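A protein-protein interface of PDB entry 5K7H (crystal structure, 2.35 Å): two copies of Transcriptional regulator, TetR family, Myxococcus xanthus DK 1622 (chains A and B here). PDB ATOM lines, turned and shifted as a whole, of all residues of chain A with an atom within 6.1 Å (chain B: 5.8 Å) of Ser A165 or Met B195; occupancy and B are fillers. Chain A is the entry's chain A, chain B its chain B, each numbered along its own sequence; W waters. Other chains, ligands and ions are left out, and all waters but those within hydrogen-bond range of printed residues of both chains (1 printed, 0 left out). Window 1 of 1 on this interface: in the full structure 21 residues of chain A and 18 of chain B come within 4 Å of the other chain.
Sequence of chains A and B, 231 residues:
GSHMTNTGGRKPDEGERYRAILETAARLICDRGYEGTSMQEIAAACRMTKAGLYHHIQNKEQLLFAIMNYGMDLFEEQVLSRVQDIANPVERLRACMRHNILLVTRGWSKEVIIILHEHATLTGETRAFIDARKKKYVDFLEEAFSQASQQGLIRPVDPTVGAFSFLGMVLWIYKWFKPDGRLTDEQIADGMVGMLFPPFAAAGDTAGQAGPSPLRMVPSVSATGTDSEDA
Of chain B, only Met B169 (3.4 Å), Met B192 (3.6 Å) and Met B195 (3.1 Å) come within 4 Å of Ser A165. Of chain A, only Val A157 (3.9 Å), Val A161 (3.8 Å), Gly A162 (3.9 Å), Ser A165 (3.1 Å) and Leu A196 (3.8 Å) come within 4 Å of Met B195. Of the printed residues of chain B, Val A157 touches Met B195 (3.9 Å). Printed residues of chain B within 4 Å of Arg A155: Gly B194 (3.8 Å) and Pro B198 (3.3 Å). Of the printed residues of chain A, Gly B168 touches Gly A168 (3.4 Å). Printed residues of chain B within 4 Å of Leu A196: Met B195 (3.8 Å). Of the printed residues of chain A, Leu B196 touches Met A169 (3.3 Å) and Met A195 (3.7 Å). The nearest residue of chain A that does not touch Met B195 is Met A195 (4.05 Å). The nearest printed residue of chain A that does not touch Gly B194 is Pro A156 (6.4 Å).
Arg A155 touches Gly B194 (CD to O, 3.8 Å). Val A157 touches Met B195. Val A161 touches Met B192. O of Val A161 touches CE of Met B195, 3.8 Å away. Met B169 touches Ser A165. Met B192 touches Ser A165 (CE to OG, 3.6 Å). Ser A165 touches Met B195 (OG to CE, 3.1 Å). Gly A168 touches Gly B168 (CA to O, 3.4 Å). Met B169 touches Met A169. SD of Met B195 touches CD1 of Leu A196, at 3.8 Å.
Gly A168 touches its own counterpart, Gly B168. Met A169 touches its own counterpart, Met B169. Met A169 touches Leu B196, but with the chains exchanged Leu A196 does not touch Met B169 (5.3 Å). Met A195 touches Leu B196, and with the chains exchanged Leu A196 touches Met B195. Positions printed for both chains: 168, 169, 195, 196 and 198.
Hydrophobic or aromatic side chains of chain B within 4 Å of the printed part of chain A: Met B169, Met B192, Met B195, Leu B196 and Pro B198. Hydrophobic or aromatic side chains of chain A that line the printed part of chain B: Val A157, Val A161, Met A169, Met A195 and Leu A196. Among the printed residues, 14 pairs touch across the chains. Among the printed residues, no Asp or Glu carboxylate lies within 4 Å of a Lys or Arg side-chain nitrogen of the other chain.
The backbone carbonyl oxygen (O) of Val A161 is in hydrogen-bond range of the side-chain hydroxyl (OG) of Ser A165 (2.7 Å).
Water W1 lies within hydrogen-bond range of O of Phe A164 and O of Met B169.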
ATOM      1  N   MET A  97      12.678  -0.991 -17.438  1.00  0.00           N
ATOM      2  CA  MET A  97      13.318  -2.279 -17.195  1.00  0.00           C
ATOM      3  C   MET A  97      13.651  -2.454 -15.715  1.00  0.00           C
ATOM      4  O   MET A  97      13.391  -3.512 -15.134  1.00  0.00           O
ATOM      5  CB  MET A  97      14.574  -2.405 -18.057  1.00  0.00           C
ATOM      6  CG  MET A  97      15.421  -3.633 -17.761  1.00  0.00           C
ATOM      7  SD  MET A  97      16.607  -3.980 -19.080  1.00  0.00           S
ATOM      8  CE  MET A  97      15.527  -4.690 -20.319  1.00  0.00           C
ATOM      9  N   PHE A 145      10.692   2.034 -28.253  1.00  0.00           N
ATOM     10  CA  PHE A 145      11.747   1.575 -29.153  1.00  0.00           C
ATOM     11  C   PHE A 145      11.726   2.356 -30.458  1.00  0.00           C
ATOM     12  O   PHE A 145      12.778   2.752 -30.972  1.00  0.00           O
ATOM     13  CB  PHE A 145      11.600   0.077 -29.428  1.00  0.00           C
ATOM     14  CG  PHE A 145      12.247  -0.799 -28.394  1.00  0.00           C
ATOM     15  CD1 PHE A 145      13.612  -1.025 -28.418  1.00  0.00           C
ATOM     16  CD2 PHE A 145      11.491  -1.402 -27.404  1.00  0.00           C
ATOM     17  CE1 PHE A 145      14.214  -1.831 -27.471  1.00  0.00           C
ATOM     18  CE2 PHE A 145      12.086  -2.210 -26.452  1.00  0.00           C
ATOM     19  CZ  PHE A 145      13.450  -2.425 -26.486  1.00  0.00           C
ATOM     20  N   ARG A 155      20.630   1.687 -31.211  1.00  0.00           N
ATOM     21  CA  ARG A 155      20.828   1.113 -32.528  1.00  0.00           C
ATOM     22  C   ARG A 155      19.476   0.725 -33.119  1.00  0.00           C
ATOM     23  O   ARG A 155      18.644   0.129 -32.417  1.00  0.00           O
ATOM     24  CB  ARG A 155      21.747  -0.106 -32.457  1.00  0.00           C
ATOM     25  CG  ARG A 155      22.167  -0.646 -33.821  1.00  0.00           C
ATOM     26  CD  ARG A 155      23.151  -1.799 -33.686  1.00  0.00           C
ATOM     27  NE  ARG A 155      24.203  -1.497 -32.719  1.00  0.00           N
ATOM     28  CZ  ARG A 155      25.317  -0.824 -32.996  1.00  0.00           C
ATOM     29  NH1 ARG A 155      25.549  -0.377 -34.225  1.00  0.00           N
ATOM     30  NH2 ARG A 155      26.206  -0.598 -32.038  1.00  0.00           N
ATOM     31  N   PRO A 156      19.203   1.051 -34.379  1.00  0.00           N
ATOM     32  CA  PRO A 156      17.886   0.749 -34.950  1.00  0.00           C
ATOM     33  C   PRO A 156      17.533  -0.728 -34.813  1.00  0.00           C
ATOM     34  O   PRO A 156      18.384  -1.608 -34.967  1.00  0.00           O
ATOM     35  CB  PRO A 156      18.024   1.163 -36.416  1.00  0.00           C
ATOM     36  CG  PRO A 156      19.091   2.192 -36.414  1.00  0.00           C
ATOM     37  CD  PRO A 156      20.057   1.775 -35.342  1.00  0.00           C
ATOM     38  N   VAL A 157      16.263  -0.984 -34.518  1.00  0.00           N
ATOM     39  CA  VAL A 157      15.741  -2.341 -34.405  1.00  0.00           C
ATOM     40  C   VAL A 157      14.231  -2.251 -34.551  1.00  0.00           C
ATOM     41  O   VAL A 157      13.618  -1.252 -34.171  1.00  0.00           O
ATOM     42  CB  VAL A 157      16.153  -2.997 -33.062  1.00  0.00           C
ATOM     43  CG1 VAL A 157      15.631  -2.183 -31.883  1.00  0.00           C
ATOM     44  CG2 VAL A 157      15.652  -4.435 -32.991  1.00  0.00           C
ATOM     45  N   THR A 160       8.861  -4.267 -32.539  1.00  0.00           N
ATOM     46  CA  THR A 160       8.323  -5.508 -31.990  1.00  0.00           C
ATOM     47  C   THR A 160       9.439  -6.420 -31.499  1.00  0.00           C
ATOM     48  O   THR A 160       9.317  -7.042 -30.437  1.00  0.00           O
ATOM     49  CB  THR A 160       7.466  -6.219 -33.040  1.00  0.00           C
ATOM     50  OG1 THR A 160       6.333  -5.404 -33.361  1.00  0.00           O
ATOM     51  CG2 THR A 160       6.978  -7.574 -32.527  1.00  0.00           C
ATOM     52  N   VAL A 161      10.534  -6.516 -32.256  1.00  0.00           N
ATOM     53  CA  VAL A 161      11.671  -7.319 -31.819  1.00  0.00           C
ATOM     54  C   VAL A 161      12.236  -6.767 -30.517  1.00  0.00           C
ATOM     55  O   VAL A 161      12.566  -7.521 -29.594  1.00  0.00           O
ATOM     56  CB  VAL A 161      12.741  -7.378 -32.925  1.00  0.00           C
ATOM     57  CG1 VAL A 161      14.000  -8.082 -32.429  1.00  0.00           C
ATOM     58  CG2 VAL A 161      12.192  -8.086 -34.155  1.00  0.00           C
ATOM     59  N   GLY A 162      12.355  -5.442 -30.421  1.00  0.00           N
ATOM     60  CA  GLY A 162      12.867  -4.846 -29.198  1.00  0.00           C
ATOM     61  C   GLY A 162      11.956  -5.085 -28.009  1.00  0.00           C
ATOM     62  O   GLY A 162      12.421  -5.403 -26.911  1.00  0.00           O
ATOM     63  N   ALA A 163      10.645  -4.936 -28.208  1.00  0.00           N
ATOM     64  CA  ALA A 163       9.702  -5.096 -27.105  1.00  0.00           C
ATOM     65  C   ALA A 163       9.759  -6.505 -26.529  1.00  0.00           C
ATOM     66  O   ALA A 163       9.807  -6.687 -25.307  1.00  0.00           O
ATOM     67  CB  ALA A 163       8.286  -4.768 -27.576  1.00  0.00           C
ATOM     68  N   PHE A 164       9.743  -7.523 -27.393  1.00  0.00           N
ATOM     69  CA  PHE A 164       9.708  -8.899 -26.914  1.00  0.00           C
ATOM     70  C   PHE A 164      11.075  -9.410 -26.486  1.00  0.00           C
ATOM     71  O   PHE A 164      11.146 -10.425 -25.786  1.00  0.00           O
ATOM     72  CB  PHE A 164       9.113  -9.815 -27.985  1.00  0.00           C
ATOM     73  CG  PHE A 164       7.626  -9.665 -28.142  1.00  0.00           C
ATOM     74  CD1 PHE A 164       6.780  -9.885 -27.065  1.00  0.00           C
ATOM     75  CD2 PHE A 164       7.071  -9.306 -29.360  1.00  0.00           C
ATOM     76  CE1 PHE A 164       5.411  -9.747 -27.199  1.00  0.00           C
ATOM     77  CE2 PHE A 164       5.701  -9.169 -29.500  1.00  0.00           C
ATOM     78  CZ  PHE A 164       4.871  -9.389 -28.417  1.00  0.00           C
ATOM     79  N   SER A 165      12.156  -8.740 -26.886  1.00  0.00           N
ATOM     80  CA  SER A 165      13.452  -9.008 -26.276  1.00  0.00           C
ATOM     81  C   SER A 165      13.503  -8.436 -24.867  1.00  0.00           C
ATOM     82  O   SER A 165      13.935  -9.109 -23.923  1.00  0.00           O
ATOM     83  CB  SER A 165      14.569  -8.423 -27.140  1.00  0.00           C
ATOM     84  OG  SER A 165      14.554  -8.993 -28.436  1.00  0.00           O
ATOM     85  N   PHE A 166      13.072  -7.183 -24.715  1.00  0.00           N
ATOM     86  CA  PHE A 166      12.865  -6.594 -23.395  1.00  0.00           C
ATOM     87  C   PHE A 166      12.091  -7.547 -22.491  1.00  0.00           C
ATOM     88  O   PHE A 166      12.553  -7.908 -21.403  1.00  0.00           O
ATOM     89  CB  PHE A 166      12.125  -5.262 -23.563  1.00  0.00           C
ATOM     90  CG  PHE A 166      11.895  -4.497 -22.285  1.00  0.00           C
ATOM     91  CD1 PHE A 166      10.962  -4.924 -21.354  1.00  0.00           C
ATOM     92  CD2 PHE A 166      12.580  -3.317 -22.041  1.00  0.00           C
ATOM     93  CE1 PHE A 166      10.742  -4.209 -20.192  1.00  0.00           C
ATOM     94  CE2 PHE A 166      12.361  -2.597 -20.885  1.00  0.00           C
ATOM     95  CZ  PHE A 166      11.441  -3.042 -19.959  1.00  0.00           C
ATOM     96  N   LEU A 167      10.908  -7.976 -22.938  1.00  0.00           N
ATOM     97  CA  LEU A 167      10.044  -8.793 -22.088  1.00  0.00           C
ATOM     98  C   LEU A 167      10.647 -10.168 -21.834  1.00  0.00           C
ATOM     99  O   LEU A 167      10.518 -10.711 -20.731  1.00  0.00           O
ATOM    100  CB  LEU A 167       8.660  -8.919 -22.725  1.00  0.00           C
ATOM    101  CG  LEU A 167       7.830  -7.633 -22.725  1.00  0.00           C
ATOM    102  CD1 LEU A 167       6.623  -7.753 -23.645  1.00  0.00           C
ATOM    103  CD2 LEU A 167       7.385  -7.285 -21.313  1.00  0.00           C
ATOM    104  N   GLY A 168      11.302 -10.753 -22.839  1.00  0.00           N
ATOM    105  CA  GLY A 168      11.933 -12.048 -22.638  1.00  0.00           C
ATOM    106  C   GLY A 168      13.009 -12.004 -21.569  1.00  0.00           C
ATOM    107  O   GLY A 168      13.031 -12.834 -20.657  1.00  0.00           O
ATOM    108  N   MET A 169      13.916 -11.030 -21.668  1.00  0.00           N
ATOM    109  CA  MET A 169      14.940 -10.849 -20.645  1.00  0.00           C
ATOM    110  C   MET A 169      14.316 -10.735 -19.261  1.00  0.00           C
ATOM    111  O   MET A 169      14.638 -11.498 -18.345  1.00  0.00           O
ATOM    112  CB  MET A 169      15.759  -9.591 -20.933  1.00  0.00           C
ATOM    113  CG  MET A 169      16.669  -9.652 -22.125  1.00  0.00           C
ATOM    114  SD  MET A 169      17.687  -8.166 -22.139  1.00  0.00           S
ATOM    115  CE  MET A 169      18.530  -8.346 -23.701  1.00  0.00           C
ATOM    116  N   VAL A 170      13.417  -9.765 -19.101  1.00  0.00           N
ATOM    117  CA  VAL A 170      12.924  -9.402 -17.776  1.00  0.00           C
ATOM    118  C   VAL A 170      12.127 -10.548 -17.169  1.00  0.00           C
ATOM    119  O   VAL A 170      12.402 -10.989 -16.046  1.00  0.00           O
ATOM    120  CB  VAL A 170      12.090  -8.110 -17.865  1.00  0.00           C
ATOM    121  CG1 VAL A 170      11.441  -7.782 -16.530  1.00  0.00           C
ATOM    122  CG2 VAL A 170      12.963  -6.954 -18.329  1.00  0.00           C
ATOM    123  N   MET A 195      23.366  -3.769 -21.052  1.00  0.00           N
ATOM    124  CA  MET A 195      23.567  -4.675 -22.178  1.00  0.00           C
ATOM    125  C   MET A 195      22.582  -4.410 -23.308  1.00  0.00           C
ATOM    126  O   MET A 195      22.931  -4.577 -24.481  1.00  0.00           O
ATOM    127  CB  MET A 195      23.441  -6.121 -21.696  1.00  0.00           C
ATOM    128  CG  MET A 195      23.481  -7.171 -22.789  1.00  0.00           C
ATOM    129  SD  MET A 195      23.712  -8.829 -22.110  1.00  0.00           S
ATOM    130  CE  MET A 195      22.402  -8.891 -20.887  1.00  0.00           C
ATOM    131  N   LEU A 196      21.359  -3.995 -22.981  1.00  0.00           N
ATOM    132  CA  LEU A 196      20.339  -3.733 -23.988  1.00  0.00           C
ATOM    133  C   LEU A 196      20.192  -2.256 -24.326  1.00  0.00           C
ATOM    134  O   LEU A 196      19.744  -1.930 -25.429  1.00  0.00           O
ATOM    135  CB  LEU A 196      18.985  -4.274 -23.513  1.00  0.00           C
ATOM    136  CG  LEU A 196      17.861  -4.322 -24.549  1.00  0.00           C
ATOM    137  CD1 LEU A 196      18.208  -5.254 -25.705  1.00  0.00           C
ATOM    138  CD2 LEU A 196      16.565  -4.757 -23.886  1.00  0.00           C
ATOM    139  N   PRO A 198      22.846   0.438 -23.868  1.00  0.00           N
ATOM    140  CA  PRO A 198      24.118   1.075 -23.531  1.00  0.00           C
ATOM    141  C   PRO A 198      24.151   2.511 -24.018  1.00  0.00           C
ATOM    142  O   PRO A 198      23.231   2.958 -24.722  1.00  0.00           O
ATOM    143  CB  PRO A 198      25.150   0.211 -24.270  1.00  0.00           C
ATOM    144  CG  PRO A 198      24.403  -0.329 -25.439  1.00  0.00           C
ATOM    145  CD  PRO A 198      22.991  -0.542 -24.961  1.00  0.00           C
ATOM    146  N   GLY B 168      16.472 -15.761 -22.208  1.00  0.00           N
ATOM    147  CA  GLY B 168      15.166 -15.129 -22.100  1.00  0.00           C
ATOM    148  C   GLY B 168      14.672 -14.597 -23.431  1.00  0.00           C
ATOM    149  O   GLY B 168      13.537 -14.855 -23.836  1.00  0.00           O
ATOM    150  N   MET B 169      15.523 -13.847 -24.134  1.00  0.00           N
ATOM    151  CA  MET B 169      15.163 -13.341 -25.455  1.00  0.00           C
ATOM    152  C   MET B 169      14.757 -14.476 -26.385  1.00  0.00           C
ATOM    153  O   MET B 169      13.693 -14.439 -27.012  1.00  0.00           O
ATOM    154  CB  MET B 169      16.338 -12.579 -26.066  1.00  0.00           C
ATOM    155  CG  MET B 169      16.645 -11.237 -25.438  1.00  0.00           C
ATOM    156  SD  MET B 169      18.120 -10.506 -26.176  1.00  0.00           S
ATOM    157  CE  MET B 169      17.630 -10.357 -27.895  1.00  0.00           C
ATOM    158  N   ASP B 190      18.049 -11.618 -36.947  1.00  0.00           N
ATOM    159  CA  ASP B 190      18.920 -10.494 -37.276  1.00  0.00           C
ATOM    160  C   ASP B 190      18.783  -9.380 -36.246  1.00  0.00           C
ATOM    161  O   ASP B 190      19.782  -8.859 -35.738  1.00  0.00           O
ATOM    162  CB  ASP B 190      18.597  -9.974 -38.677  1.00  0.00           C
ATOM    163  CG  ASP B 190      18.837 -11.015 -39.754  1.00  0.00           C
ATOM    164  OD1 ASP B 190      19.680 -11.911 -39.539  1.00  0.00           O
ATOM    165  OD2 ASP B 190      18.182 -10.934 -40.816  1.00  0.00           O
ATOM    166  N   GLY B 191      17.545  -9.002 -35.923  1.00  0.00           N
ATOM    167  CA  GLY B 191      17.338  -7.934 -34.960  1.00  0.00           C
ATOM    168  C   GLY B 191      17.884  -8.267 -33.586  1.00  0.00           C
ATOM    169  O   GLY B 191      18.526  -7.432 -32.943  1.00  0.00           O
ATOM    170  N   MET B 192      17.642  -9.493 -33.113  1.00  0.00           N
ATOM    171  CA  MET B 192      18.092  -9.867 -31.777  1.00  0.00           C
ATOM    172  C   MET B 192      19.612  -9.918 -31.699  1.00  0.00           C
ATOM    173  O   MET B 192      20.202  -9.485 -30.702  1.00  0.00           O
ATOM    174  CB  MET B 192      17.489 -11.211 -31.375  1.00  0.00           C
ATOM    175  CG  MET B 192      15.996 -11.160 -31.117  1.00  0.00           C
ATOM    176  SD  MET B 192      15.414 -12.599 -30.203  1.00  0.00           S
ATOM    177  CE  MET B 192      13.701 -12.150 -29.933  1.00  0.00           C
ATOM    178  N   VAL B 193      20.264 -10.448 -32.737  1.00  0.00           N
ATOM    179  CA  VAL B 193      21.725 -10.487 -32.754  1.00  0.00           C
ATOM    180  C   VAL B 193      22.293  -9.075 -32.708  1.00  0.00           C
ATOM    181  O   VAL B 193      23.267  -8.803 -31.996  1.00  0.00           O
ATOM    182  CB  VAL B 193      22.223 -11.264 -33.989  1.00  0.00           C
ATOM    183  CG1 VAL B 193      23.724 -11.079 -34.187  1.00  0.00           C
ATOM    184  CG2 VAL B 193      21.895 -12.742 -33.849  1.00  0.00           C
ATOM    185  N   GLY B 194      21.694  -8.151 -33.465  1.00  0.00           N
ATOM    186  CA  GLY B 194      22.204  -6.791 -33.506  1.00  0.00           C
ATOM    187  C   GLY B 194      22.030  -6.043 -32.201  1.00  0.00           C
ATOM    188  O   GLY B 194      22.808  -5.134 -31.896  1.00  0.00           O
ATOM    189  N   MET B 195      21.015  -6.404 -31.415  1.00  0.00           N
ATOM    190  CA  MET B 195      20.789  -5.741 -30.135  1.00  0.00           C
ATOM    191  C   MET B 195      21.781  -6.213 -29.083  1.00  0.00           C
ATOM    192  O   MET B 195      22.427  -5.399 -28.414  1.00  0.00           O
ATOM    193  CB  MET B 195      19.361  -5.997 -29.652  1.00  0.00           C
ATOM    194  CG  MET B 195      18.333  -5.014 -30.164  1.00  0.00           C
ATOM    195  SD  MET B 195      16.808  -5.124 -29.207  1.00  0.00           S
ATOM    196  CE  MET B 195      16.269  -6.769 -29.649  1.00  0.00           C
ATOM    197  N   LEU B 196      21.911  -7.530 -28.922  1.00  0.00           N
ATOM    198  CA  LEU B 196      22.723  -8.079 -27.844  1.00  0.00           C
ATOM    199  C   LEU B 196      24.201  -8.133 -28.206  1.00  0.00           C
ATOM    200  O   LEU B 196      25.055  -8.007 -27.320  1.00  0.00           O
ATOM    201  CB  LEU B 196      22.222  -9.479 -27.488  1.00  0.00           C
ATOM    202  CG  LEU B 196      22.275  -9.888 -26.016  1.00  0.00           C
ATOM    203  CD1 LEU B 196      21.366  -9.009 -25.171  1.00  0.00           C
ATOM    204  CD2 LEU B 196      21.886 -11.348 -25.869  1.00  0.00           C
ATOM    205  N   PHE B 197      24.523  -8.314 -29.484  1.00  0.00           N
ATOM    206  CA  PHE B 197      25.904  -8.487 -29.933  1.00  0.00           C
ATOM    207  C   PHE B 197      26.188  -7.561 -31.111  1.00  0.00           C
ATOM    208  O   PHE B 197      26.433  -8.012 -32.233  1.00  0.00           O
ATOM    209  CB  PHE B 197      26.160  -9.945 -30.310  1.00  0.00           C
ATOM    210  CG  PHE B 197      25.729 -10.926 -29.258  1.00  0.00           C
ATOM    211  CD1 PHE B 197      26.399 -11.004 -28.049  1.00  0.00           C
ATOM    212  CD2 PHE B 197      24.660 -11.779 -29.483  1.00  0.00           C
ATOM    213  CE1 PHE B 197      26.008 -11.911 -27.081  1.00  0.00           C
ATOM    214  CE2 PHE B 197      24.265 -12.689 -28.519  1.00  0.00           C
ATOM    215  CZ  PHE B 197      24.941 -12.755 -27.316  1.00  0.00           C
ATOM    216  N   PRO B 198      26.160  -6.252 -30.889  1.00  0.00           N
ATOM    217  CA  PRO B 198      26.471  -5.314 -31.964  1.00  0.00           C
ATOM    218  C   PRO B 198      27.970  -5.214 -32.174  1.00  0.00           C
ATOM    219  O   PRO B 198      28.754  -5.715 -31.352  1.00  0.00           O
ATOM    220  CB  PRO B 198      25.889  -3.991 -31.452  1.00  0.00           C
ATOM    221  CG  PRO B 198      26.023  -4.098 -29.970  1.00  0.00           C
ATOM    222  CD  PRO B 198      25.809  -5.555 -29.637  1.00  0.00           C
HETATM  223  O   HOH W   1      11.466 -12.699 -27.487  1.00  0.00           O
